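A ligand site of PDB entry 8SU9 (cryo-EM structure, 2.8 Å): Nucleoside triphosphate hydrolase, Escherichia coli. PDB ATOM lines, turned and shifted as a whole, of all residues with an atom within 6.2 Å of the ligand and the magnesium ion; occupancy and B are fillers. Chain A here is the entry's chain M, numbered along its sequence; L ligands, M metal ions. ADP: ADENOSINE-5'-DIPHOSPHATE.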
ATOM      1  N   SER A 178       3.215  -3.631 -32.499  1.00  0.00           N
ATOM      2  CA  SER A 178       4.569  -3.916 -32.946  1.00  0.00           C
ATOM      3  C   SER A 178       5.566  -3.633 -31.832  1.00  0.00           C
ATOM      4  O   SER A 178       5.201  -3.273 -30.706  1.00  0.00           O
ATOM      5  CB  SER A 178       4.889  -3.100 -34.192  1.00  0.00           C
ATOM      6  OG  SER A 178       4.244  -3.621 -35.335  1.00  0.00           O
ATOM      7  N   THR A 179       6.850  -3.799 -32.135  1.00  0.00           N
ATOM      8  CA  THR A 179       7.888  -3.618 -31.129  1.00  0.00           C
ATOM      9  C   THR A 179       8.204  -2.152 -30.932  1.00  0.00           C
ATOM     10  O   THR A 179       8.301  -1.382 -31.895  1.00  0.00           O
ATOM     11  CB  THR A 179       9.153  -4.377 -31.542  1.00  0.00           C
ATOM     12  OG1 THR A 179       8.787  -5.675 -32.042  1.00  0.00           O
ATOM     13  CG2 THR A 179      10.067  -4.553 -30.353  1.00  0.00           C
ATOM     14  N   GLY A 180       8.381  -1.754 -29.674  1.00  0.00           N
ATOM     15  CA  GLY A 180       8.747  -0.386 -29.357  1.00  0.00           C
ATOM     16  C   GLY A 180       7.674   0.643 -29.544  1.00  0.00           C
ATOM     17  O   GLY A 180       7.955   1.764 -29.983  1.00  0.00           O
ATOM     18  N   TYR A 181       6.421   0.311 -29.216  1.00  0.00           N
ATOM     19  CA  TYR A 181       5.311   1.240 -29.398  1.00  0.00           C
ATOM     20  C   TYR A 181       4.420   1.388 -28.172  1.00  0.00           C
ATOM     21  O   TYR A 181       3.534   2.246 -28.186  1.00  0.00           O
ATOM     22  CB  TYR A 181       4.464   0.825 -30.603  1.00  0.00           C
ATOM     23  CG  TYR A 181       5.016   1.335 -31.914  1.00  0.00           C
ATOM     24  CD1 TYR A 181       4.806   2.640 -32.319  1.00  0.00           C
ATOM     25  CD2 TYR A 181       5.775   0.516 -32.749  1.00  0.00           C
ATOM     26  CE1 TYR A 181       5.303   3.120 -33.504  1.00  0.00           C
ATOM     27  CE2 TYR A 181       6.289   0.994 -33.940  1.00  0.00           C
ATOM     28  CZ  TYR A 181       6.051   2.295 -34.313  1.00  0.00           C
ATOM     29  OH  TYR A 181       6.553   2.765 -35.498  1.00  0.00           O
ATOM     30  N   GLY A 182       4.632   0.606 -27.112  1.00  0.00           N
ATOM     31  CA  GLY A 182       3.943   0.877 -25.868  1.00  0.00           C
ATOM     32  C   GLY A 182       3.023  -0.199 -25.313  1.00  0.00           C
ATOM     33  O   GLY A 182       2.018   0.131 -24.671  1.00  0.00           O
ATOM     34  N   LYS A 183       3.341  -1.473 -25.535  1.00  0.00           N
ATOM     35  CA  LYS A 183       2.572  -2.534 -24.901  1.00  0.00           C
ATOM     36  C   LYS A 183       2.892  -2.642 -23.405  1.00  0.00           C
ATOM     37  O   LYS A 183       1.974  -2.735 -22.573  1.00  0.00           O
ATOM     38  CB  LYS A 183       2.848  -3.863 -25.601  1.00  0.00           C
ATOM     39  CG  LYS A 183       2.382  -3.917 -27.044  1.00  0.00           C
ATOM     40  CD  LYS A 183       2.351  -5.337 -27.564  1.00  0.00           C
ATOM     41  CE  LYS A 183       3.738  -5.927 -27.659  1.00  0.00           C
ATOM     42  NZ  LYS A 183       4.600  -5.201 -28.627  1.00  0.00           N
ATOM     43  N   SER A 184       4.183  -2.614 -23.054  1.00  0.00           N
ATOM     44  CA  SER A 184       4.583  -2.803 -21.666  1.00  0.00           C
ATOM     45  C   SER A 184       4.091  -1.664 -20.782  1.00  0.00           C
ATOM     46  O   SER A 184       3.674  -1.893 -19.645  1.00  0.00           O
ATOM     47  CB  SER A 184       6.102  -2.920 -21.577  1.00  0.00           C
ATOM     48  OG  SER A 184       6.579  -3.977 -22.380  1.00  0.00           O
ATOM     49  N   ASN A 185       4.129  -0.427 -21.287  1.00  0.00           N
ATOM     50  CA  ASN A 185       3.653   0.710 -20.519  1.00  0.00           C
ATOM     51  C   ASN A 185       2.171   0.571 -20.198  1.00  0.00           C
ATOM     52  O   ASN A 185       1.748   0.785 -19.054  1.00  0.00           O
ATOM     53  CB  ASN A 185       3.922   1.998 -21.301  1.00  0.00           C
ATOM     54  CG  ASN A 185       3.466   3.238 -20.556  1.00  0.00           C
ATOM     55  OD1 ASN A 185       3.232   3.214 -19.356  1.00  0.00           O
ATOM     56  ND2 ASN A 185       3.325   4.344 -21.292  1.00  0.00           N
ATOM     57  N   PHE A 186       1.362   0.198 -21.197  1.00  0.00           N
ATOM     58  CA  PHE A 186      -0.067   0.008 -20.966  1.00  0.00           C
ATOM     59  C   PHE A 186      -0.312  -1.119 -19.977  1.00  0.00           C
ATOM     60  O   PHE A 186      -1.175  -0.999 -19.091  1.00  0.00           O
ATOM     61  CB  PHE A 186      -0.762  -0.276 -22.297  1.00  0.00           C
ATOM     62  CG  PHE A 186      -2.252  -0.384 -22.173  1.00  0.00           C
ATOM     63  CD1 PHE A 186      -3.022   0.718 -21.842  1.00  0.00           C
ATOM     64  CD2 PHE A 186      -2.893  -1.597 -22.380  1.00  0.00           C
ATOM     65  CE1 PHE A 186      -4.381   0.614 -21.727  1.00  0.00           C
ATOM     66  CE2 PHE A 186      -4.252  -1.701 -22.266  1.00  0.00           C
ATOM     67  CZ  PHE A 186      -5.011  -0.592 -21.939  1.00  0.00           C
ATOM     68  N   ASN A 209      10.937 -11.116 -19.730  1.00  0.00           N
ATOM     69  CA  ASN A 209      12.152 -10.337 -19.818  1.00  0.00           C
ATOM     70  C   ASN A 209      12.620  -9.755 -18.490  1.00  0.00           C
ATOM     71  O   ASN A 209      13.719  -9.191 -18.435  1.00  0.00           O
ATOM     72  CB  ASN A 209      11.985  -9.187 -20.823  1.00  0.00           C
ATOM     73  CG  ASN A 209      11.770  -9.673 -22.241  1.00  0.00           C
ATOM     74  OD1 ASN A 209      10.796  -9.306 -22.905  1.00  0.00           O
ATOM     75  ND2 ASN A 209      12.673 -10.518 -22.720  1.00  0.00           N
ATOM     76  N   GLU A 211      10.957  -7.265 -16.180  1.00  0.00           N
ATOM     77  CA  GLU A 211      10.790  -5.823 -16.342  1.00  0.00           C
ATOM     78  C   GLU A 211       9.905  -5.202 -15.275  1.00  0.00           C
ATOM     79  O   GLU A 211       9.990  -3.990 -15.028  1.00  0.00           O
ATOM     80  CB  GLU A 211      10.209  -5.541 -17.729  1.00  0.00           C
ATOM     81  CG  GLU A 211      11.188  -5.698 -18.875  1.00  0.00           C
ATOM     82  CD  GLU A 211      10.536  -5.489 -20.221  1.00  0.00           C
ATOM     83  OE1 GLU A 211       9.290  -5.438 -20.277  1.00  0.00           O
ATOM     84  OE2 GLU A 211      11.268  -5.384 -21.231  1.00  0.00           O
ATOM     85  N   GLU A 478       4.391 -12.428 -24.628  1.00  0.00           N
ATOM     86  CA  GLU A 478       5.019 -13.204 -25.699  1.00  0.00           C
ATOM     87  C   GLU A 478       4.258 -14.506 -25.925  1.00  0.00           C
ATOM     88  O   GLU A 478       4.839 -15.589 -26.009  1.00  0.00           O
ATOM     89  CB  GLU A 478       6.497 -13.460 -25.404  1.00  0.00           C
ATOM     90  CG  GLU A 478       7.416 -12.363 -25.888  1.00  0.00           C
ATOM     91  CD  GLU A 478       7.513 -11.206 -24.913  1.00  0.00           C
ATOM     92  OE1 GLU A 478       6.913 -11.308 -23.823  1.00  0.00           O
ATOM     93  OE2 GLU A 478       8.174 -10.196 -25.238  1.00  0.00           O
ATOM     94  N   ARG A 566       3.444   6.824 -32.051  1.00  0.00           N
ATOM     95  CA  ARG A 566       3.875   6.184 -30.818  1.00  0.00           C
ATOM     96  C   ARG A 566       2.988   6.598 -29.657  1.00  0.00           C
ATOM     97  O   ARG A 566       2.739   7.785 -29.449  1.00  0.00           O
ATOM     98  CB  ARG A 566       5.336   6.548 -30.533  1.00  0.00           C
ATOM     99  CG  ARG A 566       5.986   5.836 -29.368  1.00  0.00           C
ATOM    100  CD  ARG A 566       7.434   6.251 -29.289  1.00  0.00           C
ATOM    101  NE  ARG A 566       8.166   5.620 -28.191  1.00  0.00           N
ATOM    102  CZ  ARG A 566       9.458   5.810 -27.956  1.00  0.00           C
ATOM    103  NH1 ARG A 566      10.188   6.610 -28.717  1.00  0.00           N
ATOM    104  NH2 ARG A 566      10.030   5.182 -26.938  1.00  0.00           N
ATOM    105  N   GLY A 567       2.512   5.619 -28.898  1.00  0.00           N
ATOM    106  CA  GLY A 567       1.684   5.882 -27.739  1.00  0.00           C
ATOM    107  C   GLY A 567       0.198   6.031 -28.007  1.00  0.00           C
ATOM    108  O   GLY A 567      -0.537   6.428 -27.098  1.00  0.00           O
ATOM    109  N   ASP A 568      -0.266   5.737 -29.218  1.00  0.00           N
ATOM    110  CA  ASP A 568      -1.675   5.803 -29.563  1.00  0.00           C
ATOM    111  C   ASP A 568      -2.224   4.413 -29.853  1.00  0.00           C
ATOM    112  O   ASP A 568      -1.501   3.514 -30.299  1.00  0.00           O
ATOM    113  CB  ASP A 568      -1.908   6.712 -30.779  1.00  0.00           C
ATOM    114  CG  ASP A 568      -1.780   8.188 -30.438  1.00  0.00           C
ATOM    115  OD1 ASP A 568      -1.527   8.503 -29.257  1.00  0.00           O
ATOM    116  OD2 ASP A 568      -1.943   9.019 -31.341  1.00  0.00           O
ATOM    117  N   SER A 583      -5.057   8.546 -26.559  1.00  0.00           N
ATOM    118  CA  SER A 583      -3.659   8.875 -26.310  1.00  0.00           C
ATOM    119  C   SER A 583      -3.367   8.477 -24.864  1.00  0.00           C
ATOM    120  O   SER A 583      -3.856   9.114 -23.924  1.00  0.00           O
ATOM    121  CB  SER A 583      -3.379  10.359 -26.560  1.00  0.00           C
ATOM    122  OG  SER A 583      -1.997  10.645 -26.419  1.00  0.00           O
ATOM    123  N   ILE A 584      -2.558   7.427 -24.686  1.00  0.00           N
ATOM    124  CA  ILE A 584      -2.413   6.788 -23.374  1.00  0.00           C
ATOM    125  C   ILE A 584      -1.436   7.565 -22.504  1.00  0.00           C
ATOM    126  O   ILE A 584      -0.470   8.162 -22.990  1.00  0.00           O
ATOM    127  CB  ILE A 584      -1.976   5.328 -23.558  1.00  0.00           C
ATOM    128  CG1 ILE A 584      -2.984   4.568 -24.414  1.00  0.00           C
ATOM    129  CG2 ILE A 584      -1.826   4.623 -22.215  1.00  0.00           C
ATOM    130  CD1 ILE A 584      -2.397   3.424 -25.192  1.00  0.00           C
ATOM    131  N   ASN A 585      -1.704   7.566 -21.201  1.00  0.00           N
ATOM    132  CA  ASN A 585      -0.841   8.210 -20.224  1.00  0.00           C
ATOM    133  C   ASN A 585       0.420   7.387 -19.962  1.00  0.00           C
ATOM    134  O   ASN A 585       0.467   6.179 -20.218  1.00  0.00           O
ATOM    135  CB  ASN A 585      -1.575   8.433 -18.899  1.00  0.00           C
ATOM    136  CG  ASN A 585      -2.605   9.532 -18.983  1.00  0.00           C
ATOM    137  OD1 ASN A 585      -2.409  10.538 -19.677  1.00  0.00           O
ATOM    138  ND2 ASN A 585      -3.713   9.357 -18.275  1.00  0.00           N
ATOM    139  N   GLN A 586       1.443   8.054 -19.445  1.00  0.00           N
ATOM    140  CA  GLN A 586       2.685   7.404 -19.093  1.00  0.00           C
ATOM    141  C   GLN A 586       2.639   6.887 -17.655  1.00  0.00           C
ATOM    142  O   GLN A 586       2.079   7.541 -16.763  1.00  0.00           O
ATOM    143  CB  GLN A 586       3.872   8.362 -19.261  1.00  0.00           C
ATOM    144  CG  GLN A 586       5.219   7.714 -19.141  1.00  0.00           C
ATOM    145  CD  GLN A 586       6.353   8.711 -19.277  1.00  0.00           C
ATOM    146  OE1 GLN A 586       6.156   9.818 -19.781  1.00  0.00           O
ATOM    147  NE2 GLN A 586       7.545   8.328 -18.825  1.00  0.00           N
ATOM    148  N   LYS A 592      11.478  -1.687 -16.565  1.00  0.00           N
ATOM    149  CA  LYS A 592      12.912  -1.598 -16.818  1.00  0.00           C
ATOM    150  C   LYS A 592      13.175  -0.927 -18.158  1.00  0.00           C
ATOM    151  O   LYS A 592      12.454  -1.137 -19.135  1.00  0.00           O
ATOM    152  CB  LYS A 592      13.526  -3.007 -16.801  1.00  0.00           C
ATOM    153  CG  LYS A 592      15.036  -3.036 -16.939  1.00  0.00           C
ATOM    154  CD  LYS A 592      15.565  -4.459 -16.895  1.00  0.00           C
ATOM    155  CE  LYS A 592      17.068  -4.503 -17.095  1.00  0.00           C
ATOM    156  NZ  LYS A 592      17.603  -5.888 -17.006  1.00  0.00           N
ATOM    157  N   SER A 593      14.227  -0.113 -18.196  1.00  0.00           N
ATOM    158  CA  SER A 593      14.439   0.768 -19.339  1.00  0.00           C
ATOM    159  C   SER A 593      14.848  -0.002 -20.592  1.00  0.00           C
ATOM    160  O   SER A 593      14.098  -0.057 -21.576  1.00  0.00           O
ATOM    161  CB  SER A 593      15.501   1.825 -19.000  1.00  0.00           C
ATOM    162  OG  SER A 593      15.061   2.659 -17.934  1.00  0.00           O
HETATM  163  PB  ADP L   1       7.073  -2.402 -26.401  1.00  0.00           P
HETATM  164  O1B ADP L   1       5.590  -2.183 -26.584  1.00  0.00           O
HETATM  165  O2B ADP L   1       7.776  -2.929 -27.623  1.00  0.00           O
HETATM  166  O3B ADP L   1       7.441  -3.122 -25.136  1.00  0.00           O
HETATM  167  PA  ADP L   1       7.824  -0.246 -24.763  1.00  0.00           P
HETATM  168  O1A ADP L   1       6.467  -0.102 -24.129  1.00  0.00           O
HETATM  169  O2A ADP L   1       8.914  -0.997 -24.043  1.00  0.00           O
HETATM  170  O3A ADP L   1       7.666  -0.918 -26.214  1.00  0.00           O
HETATM  171  O5' ADP L   1       8.384   1.222 -25.108  1.00  0.00           O
HETATM  172  C5' ADP L   1       9.624   1.644 -24.536  1.00  0.00           C
HETATM  173  C4' ADP L   1       9.678   3.160 -24.396  1.00  0.00           C
HETATM  174  O4' ADP L   1       8.576   3.777 -25.076  1.00  0.00           O
HETATM  175  C3' ADP L   1       9.580   3.575 -22.940  1.00  0.00           C
HETATM  176  O3' ADP L   1      10.857   4.041 -22.475  1.00  0.00           O
HETATM  177  C2' ADP L   1       8.565   4.693 -22.889  1.00  0.00           C
HETATM  178  O2' ADP L   1       9.184   5.891 -22.404  1.00  0.00           O
HETATM  179  C1' ADP L   1       8.094   4.888 -24.317  1.00  0.00           C
HETATM  180  N9  ADP L   1       6.608   4.909 -24.349  1.00  0.00           N
HETATM  181  C8  ADP L   1       5.811   3.885 -24.689  1.00  0.00           C
HETATM  182  N7  ADP L   1       4.502   4.233 -24.609  1.00  0.00           N
HETATM  183  C5  ADP L   1       4.450   5.517 -24.214  1.00  0.00           C
HETATM  184  C6  ADP L   1       3.387   6.502 -23.926  1.00  0.00           C
HETATM  185  N6  ADP L   1       2.079   6.166 -24.059  1.00  0.00           N
HETATM  186  N1  ADP L   1       3.761   7.737 -23.538  1.00  0.00           N
HETATM  187  C2  ADP L   1       5.052   8.076 -23.401  1.00  0.00           C
HETATM  188  N3  ADP L   1       6.075   7.227 -23.638  1.00  0.00           N
HETATM  189  C4  ADP L   1       5.843   5.957 -24.040  1.00  0.00           C
HETATM  190 MG    MG M   1       7.915  -4.947 -24.422  1.00  0.00          MG
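Within 4 Å of the magnesium ion: Ser 184.
The nearest printed residue that does not touch the magnesium ion is Glu 211 (4.4 Å).
Merely in contact with the ligand: Thr 179, Asn 185 and Gly 567.
An oxygen (O2B) of the ligand sits at hydrogen-bond distance from the backbone NH (N) of Gly 180 (2.4 Å).
The backbone NH (N) of Lys 183 is in hydrogen-bond range of an oxygen (O1B) of the ligand, at 2.6 Å.
An oxygen (O1B) of the ligand lies within salt-bridge range of the side-chain amino group (NZ) of Lys 183 (3.8 Å).
The side-chain hydroxyl of Ser 184 sits close to an oxygen (O3B) of the ligand (3.0 Å).
The guanidinium group of Arg 566 sits at hydrogen-bond distance from an oxygen (O4') of the ligand (2.7 Å).
The backbone NH (N) of Gly 182 lies within hydrogen-bond range of an oxygen (O1B) of the ligand (3.0 Å).
The backbone carbonyl oxygen (O) of Ile 584 sits at hydrogen-bond distance from a nitrogen (N6) of the ligand (3.4 Å).
An oxygen (O3A) of the ligand lies within hydrogen-bond range of the backbone NH of Tyr 181 (3.5 Å).
The magnesium ion is bound by O3B of the ligand (2.0 Å).
Slightly farther from the magnesium ion lies OG of Ser 184 (2.6 Å).
O of Ser 178 lies within hydrogen-bond range of NZ of Lys 183, at 2.9 Å.
The backbone carbonyl oxygen of Gly 567 sits at hydrogen-bond distance from the backbone NH of Ile 584.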
